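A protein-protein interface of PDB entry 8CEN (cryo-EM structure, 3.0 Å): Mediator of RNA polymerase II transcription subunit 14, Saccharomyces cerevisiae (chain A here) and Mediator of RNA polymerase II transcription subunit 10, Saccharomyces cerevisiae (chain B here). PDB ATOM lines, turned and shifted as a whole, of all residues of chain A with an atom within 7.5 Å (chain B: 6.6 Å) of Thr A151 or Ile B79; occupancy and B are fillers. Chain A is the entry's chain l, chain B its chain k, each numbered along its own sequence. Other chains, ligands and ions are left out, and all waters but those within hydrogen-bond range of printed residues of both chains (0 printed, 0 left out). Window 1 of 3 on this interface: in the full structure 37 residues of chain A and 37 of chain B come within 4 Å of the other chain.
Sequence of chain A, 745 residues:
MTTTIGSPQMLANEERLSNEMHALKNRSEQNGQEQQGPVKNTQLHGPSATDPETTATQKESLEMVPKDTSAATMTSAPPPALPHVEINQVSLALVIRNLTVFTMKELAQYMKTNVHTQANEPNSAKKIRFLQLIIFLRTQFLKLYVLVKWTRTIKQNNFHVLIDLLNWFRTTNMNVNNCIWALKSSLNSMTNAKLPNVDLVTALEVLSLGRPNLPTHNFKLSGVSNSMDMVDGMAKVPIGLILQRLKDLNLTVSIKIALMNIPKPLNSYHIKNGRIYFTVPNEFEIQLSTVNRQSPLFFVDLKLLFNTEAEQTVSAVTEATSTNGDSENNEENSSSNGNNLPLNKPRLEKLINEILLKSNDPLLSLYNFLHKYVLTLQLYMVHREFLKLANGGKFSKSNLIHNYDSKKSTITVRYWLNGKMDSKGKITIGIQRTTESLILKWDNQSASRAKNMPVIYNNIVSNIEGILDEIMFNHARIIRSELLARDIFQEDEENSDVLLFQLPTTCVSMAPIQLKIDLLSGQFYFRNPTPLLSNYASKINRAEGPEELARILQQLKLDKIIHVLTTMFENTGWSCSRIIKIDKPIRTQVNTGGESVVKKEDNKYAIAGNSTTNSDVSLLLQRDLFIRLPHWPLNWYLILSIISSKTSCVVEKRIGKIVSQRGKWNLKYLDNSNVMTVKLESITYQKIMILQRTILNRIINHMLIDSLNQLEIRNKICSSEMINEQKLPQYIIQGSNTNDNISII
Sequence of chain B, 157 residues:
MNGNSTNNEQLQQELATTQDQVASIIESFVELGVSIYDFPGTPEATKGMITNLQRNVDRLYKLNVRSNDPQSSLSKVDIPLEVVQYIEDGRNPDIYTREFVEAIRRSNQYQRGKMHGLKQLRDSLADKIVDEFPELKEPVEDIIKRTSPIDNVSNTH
Printed residues of chain B within 4 Å of Asn A88: Pro B80 and Leu B81.
Printed residues of chain B within 4 Å of Val A90: Asp B78 (3.3 Å) and Ile B79 (2.6 Å).
Printed residues of chain B within 4 Å of Ser A91: Val B77.
Val A95 touches none of the printed residues of chain B.
Of chain B, only Leu B15 (3.3 Å) and Ile B79 (3.7 Å) come within 4 Å of Thr A151.
Printed residues of chain A within 4 Å of Leu B15: Thr A151 and Arg A152.
Of the printed residues of chain A, Ile B79 touches Gln A89 (3.4 Å), Val A90 (2.6 Å), Leu A92 (3.7 Å), Trp A150 (3.6 Å) and Thr A151 (3.7 Å).
The nearest residue of chain B that does not touch Thr A151 is Val B77 (4.8 Å).
The nearest residue of chain A that does not touch Ile B79 is Leu A147 (4.1 Å).
The nearest printed residue of chain B that does not touch Leu A92 is Leu B15 (5.0 Å).
Hydrophobic or aromatic side chains of chain A within 4 Å of the printed part of chain B: Val A90, Leu A92, Ala A93, Tyr A145, Leu A147, Val A148 and Trp A150.
Among the printed residues, no Asp or Glu carboxylate lies within 4 Å of a Lys or Arg side-chain nitrogen of the other chain.
O of Val A90 lies close to OD1 of Asp B78 (3.3 Å).
O of Leu B74 is in hydrogen-bond range of N of Leu A92 (3.2 Å).
O of Val B77 sits at hydrogen-bond distance from N of Leu A92.
OE1 of Gln A89 lies close to OD2 of Asp B78 (2.9 Å).
N of Lys A149 is in hydrogen-bond range of OE1 of Gln B19, at 3.4 Å.
The side-chain amide oxygen (OE1) of Gln B12 sits at hydrogen-bond distance from the side-chain amino group (NZ) of Lys A155, 3.3 Å away.
OE1 of Gln B19 lies close to O of Val A148, 3.5 Å away.
The backbone carbonyl oxygen (O) of Leu B74 sits at hydrogen-bond distance from the backbone NH (N) of Ala A93 (2.7 Å).
The backbone carbonyl oxygen of Ile B79 sits at hydrogen-bond distance from the backbone NH of Val A90 (2.6 Å).
O of Asn A88 touches CA of Pro B80, 3.8 Å away.
Asn A88 touches Leu B81 (O to CD2, 3.6 Å).
O of Ile B79 touches CA of Gln A89, at 3.4 Å.
Val B84 touches Leu A147 (CG1 to CD1, 3.7 Å).
Trp A150 touches Ile B79.
Trp A150 touches Pro B80.
Thr A151 touches Leu B15.
Arg A152 touches Gln B12.
Ile A154 touches Gln B12 (O to NE2, 3.7 Å).
Asn A157 touches Val B77 (ND2 to CA, 3.7 Å).
The backbone carbonyl oxygen (O) of Leu B15 sits at hydrogen-bond distance from the side-chain hydroxyl (OG1) of Thr B18 (2.7 Å).
The side-chain hydroxyl (OG1) of Thr A153 lies within hydrogen-bond range of the backbone carbonyl oxygen (O) of Trp A150 (2.5 Å).
The side-chain hydroxyl (OG1) of Thr A151 sits at hydrogen-bond distance from the backbone carbonyl oxygen (O) of Val A148, at 2.5 Å.
The backbone carbonyl oxygen (O) of Arg A152 is in hydrogen-bond range of the side-chain amino group (NZ) of Lys A155, 3.4 Å away.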
ATOM      1  N   ILE A  87      -7.796  31.799 -19.748  1.00  0.00           N
ATOM      2  CA  ILE A  87      -8.907  32.629 -19.294  1.00  0.00           C
ATOM      3  C   ILE A  87     -10.042  32.531 -20.303  1.00  0.00           C
ATOM      4  O   ILE A  87      -9.807  32.447 -21.515  1.00  0.00           O
ATOM      5  CB  ILE A  87      -8.451  34.088 -19.102  1.00  0.00           C
ATOM      6  CG1 ILE A  87      -7.077  34.125 -18.429  1.00  0.00           C
ATOM      7  CG2 ILE A  87      -9.465  34.871 -18.275  1.00  0.00           C
ATOM      8  CD1 ILE A  87      -6.567  35.523 -18.150  1.00  0.00           C
ATOM      9  N   ASN A  88     -11.279  32.520 -19.788  1.00  0.00           N
ATOM     10  CA  ASN A  88     -12.512  32.508 -20.585  1.00  0.00           C
ATOM     11  C   ASN A  88     -12.606  31.282 -21.493  1.00  0.00           C
ATOM     12  O   ASN A  88     -13.206  31.338 -22.569  1.00  0.00           O
ATOM     13  CB  ASN A  88     -12.666  33.796 -21.404  1.00  0.00           C
ATOM     14  CG  ASN A  88     -12.806  35.027 -20.531  1.00  0.00           C
ATOM     15  OD1 ASN A  88     -11.942  35.903 -20.529  1.00  0.00           O
ATOM     16  ND2 ASN A  88     -13.901  35.100 -19.782  1.00  0.00           N
ATOM     17  N   GLN A  89     -12.020  30.166 -21.066  1.00  0.00           N
ATOM     18  CA  GLN A  89     -12.107  28.905 -21.786  1.00  0.00           C
ATOM     19  C   GLN A  89     -12.591  27.815 -20.839  1.00  0.00           C
ATOM     20  O   GLN A  89     -12.351  27.869 -19.629  1.00  0.00           O
ATOM     21  CB  GLN A  89     -10.760  28.518 -22.414  1.00  0.00           C
ATOM     22  CG  GLN A  89      -9.645  28.269 -21.415  1.00  0.00           C
ATOM     23  CD  GLN A  89      -8.425  27.634 -22.054  1.00  0.00           C
ATOM     24  OE1 GLN A  89      -8.142  27.855 -23.230  1.00  0.00           O
ATOM     25  NE2 GLN A  89      -7.696  26.841 -21.278  1.00  0.00           N
ATOM     26  N   VAL A  90     -13.296  26.835 -21.402  1.00  0.00           N
ATOM     27  CA  VAL A  90     -13.946  25.784 -20.633  1.00  0.00           C
ATOM     28  C   VAL A  90     -13.664  24.453 -21.324  1.00  0.00           C
ATOM     29  O   VAL A  90     -13.299  24.404 -22.502  1.00  0.00           O
ATOM     30  CB  VAL A  90     -15.470  26.053 -20.494  1.00  0.00           C
ATOM     31  CG1 VAL A  90     -16.199  25.833 -21.817  1.00  0.00           C
ATOM     32  CG2 VAL A  90     -16.107  25.275 -19.339  1.00  0.00           C
ATOM     33  N   SER A  91     -13.791  23.366 -20.565  1.00  0.00           N
ATOM     34  CA  SER A  91     -13.607  22.030 -21.110  1.00  0.00           C
ATOM     35  C   SER A  91     -14.945  21.463 -21.572  1.00  0.00           C
ATOM     36  O   SER A  91     -16.006  21.780 -21.022  1.00  0.00           O
ATOM     37  CB  SER A  91     -12.963  21.101 -20.077  1.00  0.00           C
ATOM     38  OG  SER A  91     -13.908  20.658 -19.121  1.00  0.00           O
ATOM     39  N   LEU A  92     -14.891  20.629 -22.614  1.00  0.00           N
ATOM     40  CA  LEU A  92     -16.139  20.145 -23.194  1.00  0.00           C
ATOM     41  C   LEU A  92     -16.764  19.058 -22.322  1.00  0.00           C
ATOM     42  O   LEU A  92     -17.983  18.848 -22.369  1.00  0.00           O
ATOM     43  CB  LEU A  92     -15.912  19.684 -24.640  1.00  0.00           C
ATOM     44  CG  LEU A  92     -17.074  19.131 -25.481  1.00  0.00           C
ATOM     45  CD1 LEU A  92     -16.926  19.560 -26.917  1.00  0.00           C
ATOM     46  CD2 LEU A  92     -17.161  17.648 -25.444  1.00  0.00           C
ATOM     47  N   ALA A  93     -15.960  18.381 -21.497  1.00  0.00           N
ATOM     48  CA  ALA A  93     -16.527  17.567 -20.426  1.00  0.00           C
ATOM     49  C   ALA A  93     -17.363  18.420 -19.482  1.00  0.00           C
ATOM     50  O   ALA A  93     -18.454  18.014 -19.059  1.00  0.00           O
ATOM     51  CB  ALA A  93     -15.413  16.866 -19.653  1.00  0.00           C
ATOM     52  N   VAL A  95     -18.827  21.273 -20.298  1.00  0.00           N
ATOM     53  CA  VAL A  95     -20.058  21.738 -20.941  1.00  0.00           C
ATOM     54  C   VAL A  95     -21.087  20.610 -21.035  1.00  0.00           C
ATOM     55  O   VAL A  95     -22.289  20.859 -20.881  1.00  0.00           O
ATOM     56  CB  VAL A  95     -19.793  22.411 -22.311  1.00  0.00           C
ATOM     57  CG1 VAL A  95     -19.504  21.436 -23.409  1.00  0.00           C
ATOM     58  CG2 VAL A  95     -20.985  23.244 -22.733  1.00  0.00           C
ATOM     59  N   LEU A 144     -25.859  22.052 -28.787  1.00  0.00           N
ATOM     60  CA  LEU A 144     -24.781  21.154 -28.368  1.00  0.00           C
ATOM     61  C   LEU A 144     -24.297  20.296 -29.534  1.00  0.00           C
ATOM     62  O   LEU A 144     -23.092  20.057 -29.683  1.00  0.00           O
ATOM     63  CB  LEU A 144     -25.251  20.258 -27.219  1.00  0.00           C
ATOM     64  CG  LEU A 144     -24.247  19.208 -26.725  1.00  0.00           C
ATOM     65  CD1 LEU A 144     -23.108  19.850 -25.937  1.00  0.00           C
ATOM     66  CD2 LEU A 144     -24.925  18.098 -25.925  1.00  0.00           C
ATOM     67  N   TYR A 145     -25.234  19.817 -30.360  1.00  0.00           N
ATOM     68  CA  TYR A 145     -24.900  19.007 -31.527  1.00  0.00           C
ATOM     69  C   TYR A 145     -24.052  19.808 -32.512  1.00  0.00           C
ATOM     70  O   TYR A 145     -23.058  19.302 -33.049  1.00  0.00           O
ATOM     71  CB  TYR A 145     -26.202  18.534 -32.183  1.00  0.00           C
ATOM     72  CG  TYR A 145     -26.109  17.601 -33.377  1.00  0.00           C
ATOM     73  CD1 TYR A 145     -24.960  16.869 -33.648  1.00  0.00           C
ATOM     74  CD2 TYR A 145     -27.182  17.472 -34.249  1.00  0.00           C
ATOM     75  CE1 TYR A 145     -24.897  16.025 -34.734  1.00  0.00           C
ATOM     76  CE2 TYR A 145     -27.116  16.634 -35.343  1.00  0.00           C
ATOM     77  CZ  TYR A 145     -25.971  15.913 -35.580  1.00  0.00           C
ATOM     78  OH  TYR A 145     -25.895  15.073 -36.665  1.00  0.00           O
ATOM     79  N   VAL A 146     -24.426  21.068 -32.748  1.00  0.00           N
ATOM     80  CA  VAL A 146     -23.642  21.940 -33.626  1.00  0.00           C
ATOM     81  C   VAL A 146     -22.267  22.213 -33.021  1.00  0.00           C
ATOM     82  O   VAL A 146     -21.258  22.269 -33.736  1.00  0.00           O
ATOM     83  CB  VAL A 146     -24.420  23.241 -33.914  1.00  0.00           C
ATOM     84  CG1 VAL A 146     -23.587  24.215 -34.738  1.00  0.00           C
ATOM     85  CG2 VAL A 146     -25.716  22.930 -34.643  1.00  0.00           C
ATOM     86  N   LEU A 147     -22.203  22.355 -31.693  1.00  0.00           N
ATOM     87  CA  LEU A 147     -20.932  22.586 -31.008  1.00  0.00           C
ATOM     88  C   LEU A 147     -19.980  21.408 -31.187  1.00  0.00           C
ATOM     89  O   LEU A 147     -18.794  21.588 -31.487  1.00  0.00           O
ATOM     90  CB  LEU A 147     -21.199  22.839 -29.521  1.00  0.00           C
ATOM     91  CG  LEU A 147     -20.171  23.433 -28.553  1.00  0.00           C
ATOM     92  CD1 LEU A 147     -20.940  24.065 -27.414  1.00  0.00           C
ATOM     93  CD2 LEU A 147     -19.182  22.410 -28.003  1.00  0.00           C
ATOM     94  N   VAL A 148     -20.483  20.187 -31.005  1.00  0.00           N
ATOM     95  CA  VAL A 148     -19.605  19.025 -31.121  1.00  0.00           C
ATOM     96  C   VAL A 148     -19.289  18.719 -32.591  1.00  0.00           C
ATOM     97  O   VAL A 148     -18.194  18.225 -32.912  1.00  0.00           O
ATOM     98  CB  VAL A 148     -20.203  17.833 -30.338  1.00  0.00           C
ATOM     99  CG1 VAL A 148     -21.570  17.447 -30.853  1.00  0.00           C
ATOM    100  CG2 VAL A 148     -19.253  16.637 -30.333  1.00  0.00           C
ATOM    101  N   LYS A 149     -20.195  19.074 -33.512  1.00  0.00           N
ATOM    102  CA  LYS A 149     -19.852  19.072 -34.933  1.00  0.00           C
ATOM    103  C   LYS A 149     -18.707  20.035 -35.232  1.00  0.00           C
ATOM    104  O   LYS A 149     -17.809  19.719 -36.022  1.00  0.00           O
ATOM    105  CB  LYS A 149     -21.078  19.436 -35.771  1.00  0.00           C
ATOM    106  CG  LYS A 149     -20.821  19.458 -37.275  1.00  0.00           C
ATOM    107  CD  LYS A 149     -20.564  18.086 -37.870  1.00  0.00           C
ATOM    108  CE  LYS A 149     -21.823  17.240 -37.868  1.00  0.00           C
ATOM    109  NZ  LYS A 149     -22.864  17.779 -38.789  1.00  0.00           N
ATOM    110  N   TRP A 150     -18.727  21.216 -34.611  1.00  0.00           N
ATOM    111  CA  TRP A 150     -17.635  22.172 -34.768  1.00  0.00           C
ATOM    112  C   TRP A 150     -16.335  21.659 -34.158  1.00  0.00           C
ATOM    113  O   TRP A 150     -15.254  21.938 -34.689  1.00  0.00           O
ATOM    114  CB  TRP A 150     -18.033  23.516 -34.153  1.00  0.00           C
ATOM    115  CG  TRP A 150     -16.880  24.423 -33.856  1.00  0.00           C
ATOM    116  CD1 TRP A 150     -16.217  25.225 -34.734  1.00  0.00           C
ATOM    117  CD2 TRP A 150     -16.275  24.646 -32.575  1.00  0.00           C
ATOM    118  NE1 TRP A 150     -15.225  25.916 -34.084  1.00  0.00           N
ATOM    119  CE2 TRP A 150     -15.241  25.581 -32.757  1.00  0.00           C
ATOM    120  CE3 TRP A 150     -16.507  24.141 -31.295  1.00  0.00           C
ATOM    121  CZ2 TRP A 150     -14.437  26.019 -31.709  1.00  0.00           C
ATOM    122  CZ3 TRP A 150     -15.708  24.575 -30.256  1.00  0.00           C
ATOM    123  CH2 TRP A 150     -14.684  25.504 -30.468  1.00  0.00           C
ATOM    124  N   THR A 151     -16.416  20.920 -33.050  1.00  0.00           N
ATOM    125  CA  THR A 151     -15.208  20.316 -32.492  1.00  0.00           C
ATOM    126  C   THR A 151     -14.651  19.221 -33.394  1.00  0.00           C
ATOM    127  O   THR A 151     -13.440  18.970 -33.375  1.00  0.00           O
ATOM    128  CB  THR A 151     -15.458  19.750 -31.096  1.00  0.00           C
ATOM    129  OG1 THR A 151     -16.405  18.678 -31.168  1.00  0.00           O
ATOM    130  CG2 THR A 151     -15.961  20.828 -30.173  1.00  0.00           C
ATOM    131  N   ARG A 152     -15.506  18.549 -34.173  1.00  0.00           N
ATOM    132  CA  ARG A 152     -14.972  17.611 -35.163  1.00  0.00           C
ATOM    133  C   ARG A 152     -14.163  18.284 -36.269  1.00  0.00           C
ATOM    134  O   ARG A 152     -13.367  17.602 -36.924  1.00  0.00           O
ATOM    135  CB  ARG A 152     -16.064  16.781 -35.835  1.00  0.00           C
ATOM    136  CG  ARG A 152     -16.630  15.633 -35.038  1.00  0.00           C
ATOM    137  CD  ARG A 152     -17.949  15.223 -35.650  1.00  0.00           C
ATOM    138  NE  ARG A 152     -17.708  14.539 -36.917  1.00  0.00           N
ATOM    139  CZ  ARG A 152     -18.070  13.295 -37.201  1.00  0.00           C
ATOM    140  NH1 ARG A 152     -18.666  12.527 -36.309  1.00  0.00           N
ATOM    141  NH2 ARG A 152     -17.814  12.807 -38.411  1.00  0.00           N
ATOM    142  N   THR A 153     -14.361  19.585 -36.510  1.00  0.00           N
ATOM    143  CA  THR A 153     -13.639  20.259 -37.589  1.00  0.00           C
ATOM    144  C   THR A 153     -12.141  20.332 -37.306  1.00  0.00           C
ATOM    145  O   THR A 153     -11.324  20.166 -38.220  1.00  0.00           O
ATOM    146  CB  THR A 153     -14.208  21.660 -37.810  1.00  0.00           C
ATOM    147  OG1 THR A 153     -13.900  22.488 -36.682  1.00  0.00           O
ATOM    148  CG2 THR A 153     -15.716  21.599 -37.995  1.00  0.00           C
ATOM    149  N   ILE A 154     -11.764  20.574 -36.056  1.00  0.00           N
ATOM    150  CA  ILE A 154     -10.354  20.637 -35.688  1.00  0.00           C
ATOM    151  C   ILE A 154      -9.838  19.222 -35.467  1.00  0.00           C
ATOM    152  O   ILE A 154     -10.395  18.462 -34.666  1.00  0.00           O
ATOM    153  CB  ILE A 154     -10.157  21.507 -34.437  1.00  0.00           C
ATOM    154  CG1 ILE A 154     -10.742  22.901 -34.665  1.00  0.00           C
ATOM    155  CG2 ILE A 154      -8.682  21.614 -34.093  1.00  0.00           C
ATOM    156  CD1 ILE A 154     -10.105  23.652 -35.813  1.00  0.00           C
ATOM    157  N   LYS A 155      -8.771  18.864 -36.180  1.00  0.00           N
ATOM    158  CA  LYS A 155      -8.235  17.509 -36.128  1.00  0.00           C
ATOM    159  C   LYS A 155      -7.088  17.371 -35.134  1.00  0.00           C
ATOM    160  O   LYS A 155      -7.047  16.402 -34.367  1.00  0.00           O
ATOM    161  CB  LYS A 155      -7.769  17.077 -37.521  1.00  0.00           C
ATOM    162  CG  LYS A 155      -8.865  17.072 -38.575  1.00  0.00           C
ATOM    163  CD  LYS A 155     -10.062  16.240 -38.143  1.00  0.00           C
ATOM    164  CE  LYS A 155     -11.011  16.007 -39.309  1.00  0.00           C
ATOM    165  NZ  LYS A 155     -12.168  15.153 -38.927  1.00  0.00           N
ATOM    166  N   ASN A 157      -6.423  19.350 -32.611  1.00  0.00           N
ATOM    167  CA  ASN A 157      -6.803  19.947 -31.324  1.00  0.00           C
ATOM    168  C   ASN A 157      -5.809  21.031 -30.898  1.00  0.00           C
ATOM    169  O   ASN A 157      -5.346  21.078 -29.756  1.00  0.00           O
ATOM    170  CB  ASN A 157      -6.956  18.873 -30.241  1.00  0.00           C
ATOM    171  CG  ASN A 157      -7.815  19.332 -29.079  1.00  0.00           C
ATOM    172  OD1 ASN A 157      -8.537  20.324 -29.181  1.00  0.00           O
ATOM    173  ND2 ASN A 157      -7.738  18.613 -27.966  1.00  0.00           N
ATOM    174  N   PHE A 159      -6.408  24.381 -31.005  1.00  0.00           N
ATOM    175  CA  PHE A 159      -7.129  25.642 -30.899  1.00  0.00           C
ATOM    176  C   PHE A 159      -6.516  26.535 -29.826  1.00  0.00           C
ATOM    177  O   PHE A 159      -6.551  27.765 -29.949  1.00  0.00           O
ATOM    178  CB  PHE A 159      -8.606  25.380 -30.609  1.00  0.00           C
ATOM    179  CG  PHE A 159      -9.526  26.437 -31.148  1.00  0.00           C
ATOM    180  CD1 PHE A 159      -9.837  27.558 -30.398  1.00  0.00           C
ATOM    181  CD2 PHE A 159     -10.092  26.299 -32.408  1.00  0.00           C
ATOM    182  CE1 PHE A 159     -10.685  28.531 -30.900  1.00  0.00           C
ATOM    183  CE2 PHE A 159     -10.944  27.264 -32.913  1.00  0.00           C
ATOM    184  CZ  PHE A 159     -11.239  28.382 -32.158  1.00  0.00           C
ATOM    185  N   GLN B  12     -11.423  11.811 -32.239  1.00  0.00           N
ATOM    186  CA  GLN B  12     -12.339  11.666 -33.368  1.00  0.00           C
ATOM    187  C   GLN B  12     -13.396  10.596 -33.096  1.00  0.00           C
ATOM    188  O   GLN B  12     -14.587  10.808 -33.372  1.00  0.00           O
ATOM    189  CB  GLN B  12     -11.553  11.354 -34.642  1.00  0.00           C
ATOM    190  CG  GLN B  12     -10.803  12.558 -35.209  1.00  0.00           C
ATOM    191  CD  GLN B  12     -11.706  13.759 -35.442  1.00  0.00           C
ATOM    192  OE1 GLN B  12     -12.742  13.653 -36.097  1.00  0.00           O
ATOM    193  NE2 GLN B  12     -11.317  14.907 -34.897  1.00  0.00           N
ATOM    194  N   LEU B  15     -15.893  12.024 -30.354  1.00  0.00           N
ATOM    195  CA  LEU B  15     -16.815  13.003 -30.916  1.00  0.00           C
ATOM    196  C   LEU B  15     -17.840  12.350 -31.832  1.00  0.00           C
ATOM    197  O   LEU B  15     -19.011  12.731 -31.806  1.00  0.00           O
ATOM    198  CB  LEU B  15     -16.075  14.128 -31.641  1.00  0.00           C
ATOM    199  CG  LEU B  15     -14.993  14.902 -30.886  1.00  0.00           C
ATOM    200  CD1 LEU B  15     -14.474  16.073 -31.707  1.00  0.00           C
ATOM    201  CD2 LEU B  15     -15.486  15.351 -29.515  1.00  0.00           C
ATOM    202  N   THR B  18     -20.432  10.632 -29.706  1.00  0.00           N
ATOM    203  CA  THR B  18     -21.310  11.616 -29.080  1.00  0.00           C
ATOM    204  C   THR B  18     -22.246  12.271 -30.092  1.00  0.00           C
ATOM    205  O   THR B  18     -23.349  12.684 -29.712  1.00  0.00           O
ATOM    206  CB  THR B  18     -20.504  12.672 -28.325  1.00  0.00           C
ATOM    207  OG1 THR B  18     -19.509  13.236 -29.184  1.00  0.00           O
ATOM    208  CG2 THR B  18     -19.851  12.062 -27.087  1.00  0.00           C
ATOM    209  N   GLN B  19     -21.827  12.388 -31.363  1.00  0.00           N
ATOM    210  CA  GLN B  19     -22.763  12.746 -32.432  1.00  0.00           C
ATOM    211  C   GLN B  19     -23.930  11.773 -32.433  1.00  0.00           C
ATOM    212  O   GLN B  19     -25.100  12.177 -32.485  1.00  0.00           O
ATOM    213  CB  GLN B  19     -22.108  12.679 -33.817  1.00  0.00           C
ATOM    214  CG  GLN B  19     -20.893  13.523 -34.140  1.00  0.00           C
ATOM    215  CD  GLN B  19     -21.094  15.004 -34.096  1.00  0.00           C
ATOM    216  OE1 GLN B  19     -20.552  15.678 -33.233  1.00  0.00           O
ATOM    217  NE2 GLN B  19     -21.827  15.530 -35.055  1.00  0.00           N
ATOM    218  N   LEU B  74     -12.561  14.383 -23.376  1.00  0.00           N
ATOM    219  CA  LEU B  74     -13.646  15.341 -23.184  1.00  0.00           C
ATOM    220  C   LEU B  74     -13.185  16.560 -22.392  1.00  0.00           C
ATOM    221  O   LEU B  74     -13.657  17.674 -22.641  1.00  0.00           O
ATOM    222  CB  LEU B  74     -14.807  14.654 -22.452  1.00  0.00           C
ATOM    223  CG  LEU B  74     -15.922  13.763 -23.037  1.00  0.00           C
ATOM    224  CD1 LEU B  74     -16.817  14.468 -23.991  1.00  0.00           C
ATOM    225  CD2 LEU B  74     -15.386  12.507 -23.704  1.00  0.00           C
ATOM    226  N   VAL B  77     -10.065  18.537 -24.654  1.00  0.00           N
ATOM    227  CA  VAL B  77     -10.535  19.442 -25.695  1.00  0.00           C
ATOM    228  C   VAL B  77     -11.055  20.720 -25.041  1.00  0.00           C
ATOM    229  O   VAL B  77     -11.683  20.688 -23.972  1.00  0.00           O
ATOM    230  CB  VAL B  77     -11.589  18.751 -26.585  1.00  0.00           C
ATOM    231  CG1 VAL B  77     -12.776  18.285 -25.778  1.00  0.00           C
ATOM    232  CG2 VAL B  77     -12.037  19.656 -27.734  1.00  0.00           C
ATOM    233  N   ASP B  78     -10.743  21.861 -25.649  1.00  0.00           N
ATOM    234  CA  ASP B  78     -11.010  23.165 -25.059  1.00  0.00           C
ATOM    235  C   ASP B  78     -12.091  23.899 -25.836  1.00  0.00           C
ATOM    236  O   ASP B  78     -12.124  23.853 -27.070  1.00  0.00           O
ATOM    237  CB  ASP B  78      -9.741  24.016 -25.019  1.00  0.00           C
ATOM    238  CG  ASP B  78      -9.941  25.307 -24.263  1.00  0.00           C
ATOM    239  OD1 ASP B  78     -10.136  25.250 -23.032  1.00  0.00           O
ATOM    240  OD2 ASP B  78      -9.925  26.376 -24.907  1.00  0.00           O
ATOM    241  N   ILE B  79     -12.970  24.584 -25.101  1.00  0.00           N
ATOM    242  CA  ILE B  79     -14.086  25.319 -25.676  1.00  0.00           C
ATOM    243  C   ILE B  79     -14.041  26.745 -25.139  1.00  0.00           C
ATOM    244  O   ILE B  79     -13.974  26.943 -23.923  1.00  0.00           O
ATOM    245  CB  ILE B  79     -15.447  24.681 -25.343  1.00  0.00           C
ATOM    246  CG1 ILE B  79     -15.460  23.190 -25.676  1.00  0.00           C
ATOM    247  CG2 ILE B  79     -16.556  25.406 -26.091  1.00  0.00           C
ATOM    248  CD1 ILE B  79     -15.252  22.877 -27.124  1.00  0.00           C
ATOM    249  N   PRO B  80     -14.053  27.768 -25.986  1.00  0.00           N
ATOM    250  CA  PRO B  80     -14.276  29.146 -25.530  1.00  0.00           C
ATOM    251  C   PRO B  80     -15.720  29.640 -25.631  1.00  0.00           C
ATOM    252  O   PRO B  80     -16.634  28.938 -26.075  1.00  0.00           O
ATOM    253  CB  PRO B  80     -13.311  29.933 -26.479  1.00  0.00           C
ATOM    254  CG  PRO B  80     -12.792  28.739 -27.426  1.00  0.00           C
ATOM    255  CD  PRO B  80     -13.989  27.957 -27.423  1.00  0.00           C
ATOM    256  N   LEU B  81     -15.920  30.873 -25.153  1.00  0.00           N
ATOM    257  CA  LEU B  81     -17.268  31.419 -25.000  1.00  0.00           C
ATOM    258  C   LEU B  81     -17.809  32.034 -26.288  1.00  0.00           C
ATOM    259  O   LEU B  81     -19.032  32.102 -26.474  1.00  0.00           O
ATOM    260  CB  LEU B  81     -17.297  32.471 -23.882  1.00  0.00           C
ATOM    261  CG  LEU B  81     -16.702  33.872 -24.096  1.00  0.00           C
ATOM    262  CD1 LEU B  81     -17.204  34.810 -23.008  1.00  0.00           C
ATOM    263  CD2 LEU B  81     -15.175  33.896 -24.148  1.00  0.00           C
ATOM    264  N   VAL B  83     -17.576  31.025 -29.476  1.00  0.00           N
ATOM    265  CA  VAL B  83     -18.219  30.076 -30.380  1.00  0.00           C
ATOM    266  C   VAL B  83     -19.568  29.624 -29.820  1.00  0.00           C
ATOM    267  O   VAL B  83     -20.527  29.424 -30.577  1.00  0.00           O
ATOM    268  CB  VAL B  83     -17.282  28.889 -30.692  1.00  0.00           C
ATOM    269  CG1 VAL B  83     -16.951  28.084 -29.449  1.00  0.00           C
ATOM    270  CG2 VAL B  83     -17.873  27.999 -31.781  1.00  0.00           C
ATOM    271  N   VAL B  84     -19.688  29.495 -28.493  1.00  0.00           N
ATOM    272  CA  VAL B  84     -20.950  29.011 -27.940  1.00  0.00           C
ATOM    273  C   VAL B  84     -22.013  30.106 -28.007  1.00  0.00           C
ATOM    274  O   VAL B  84     -23.174  29.833 -28.341  1.00  0.00           O
ATOM    275  CB  VAL B  84     -20.763  28.434 -26.516  1.00  0.00           C
ATOM    276  CG1 VAL B  84     -19.673  27.379 -26.521  1.00  0.00           C
ATOM    277  CG2 VAL B  84     -20.493  29.482 -25.446  1.00  0.00           C
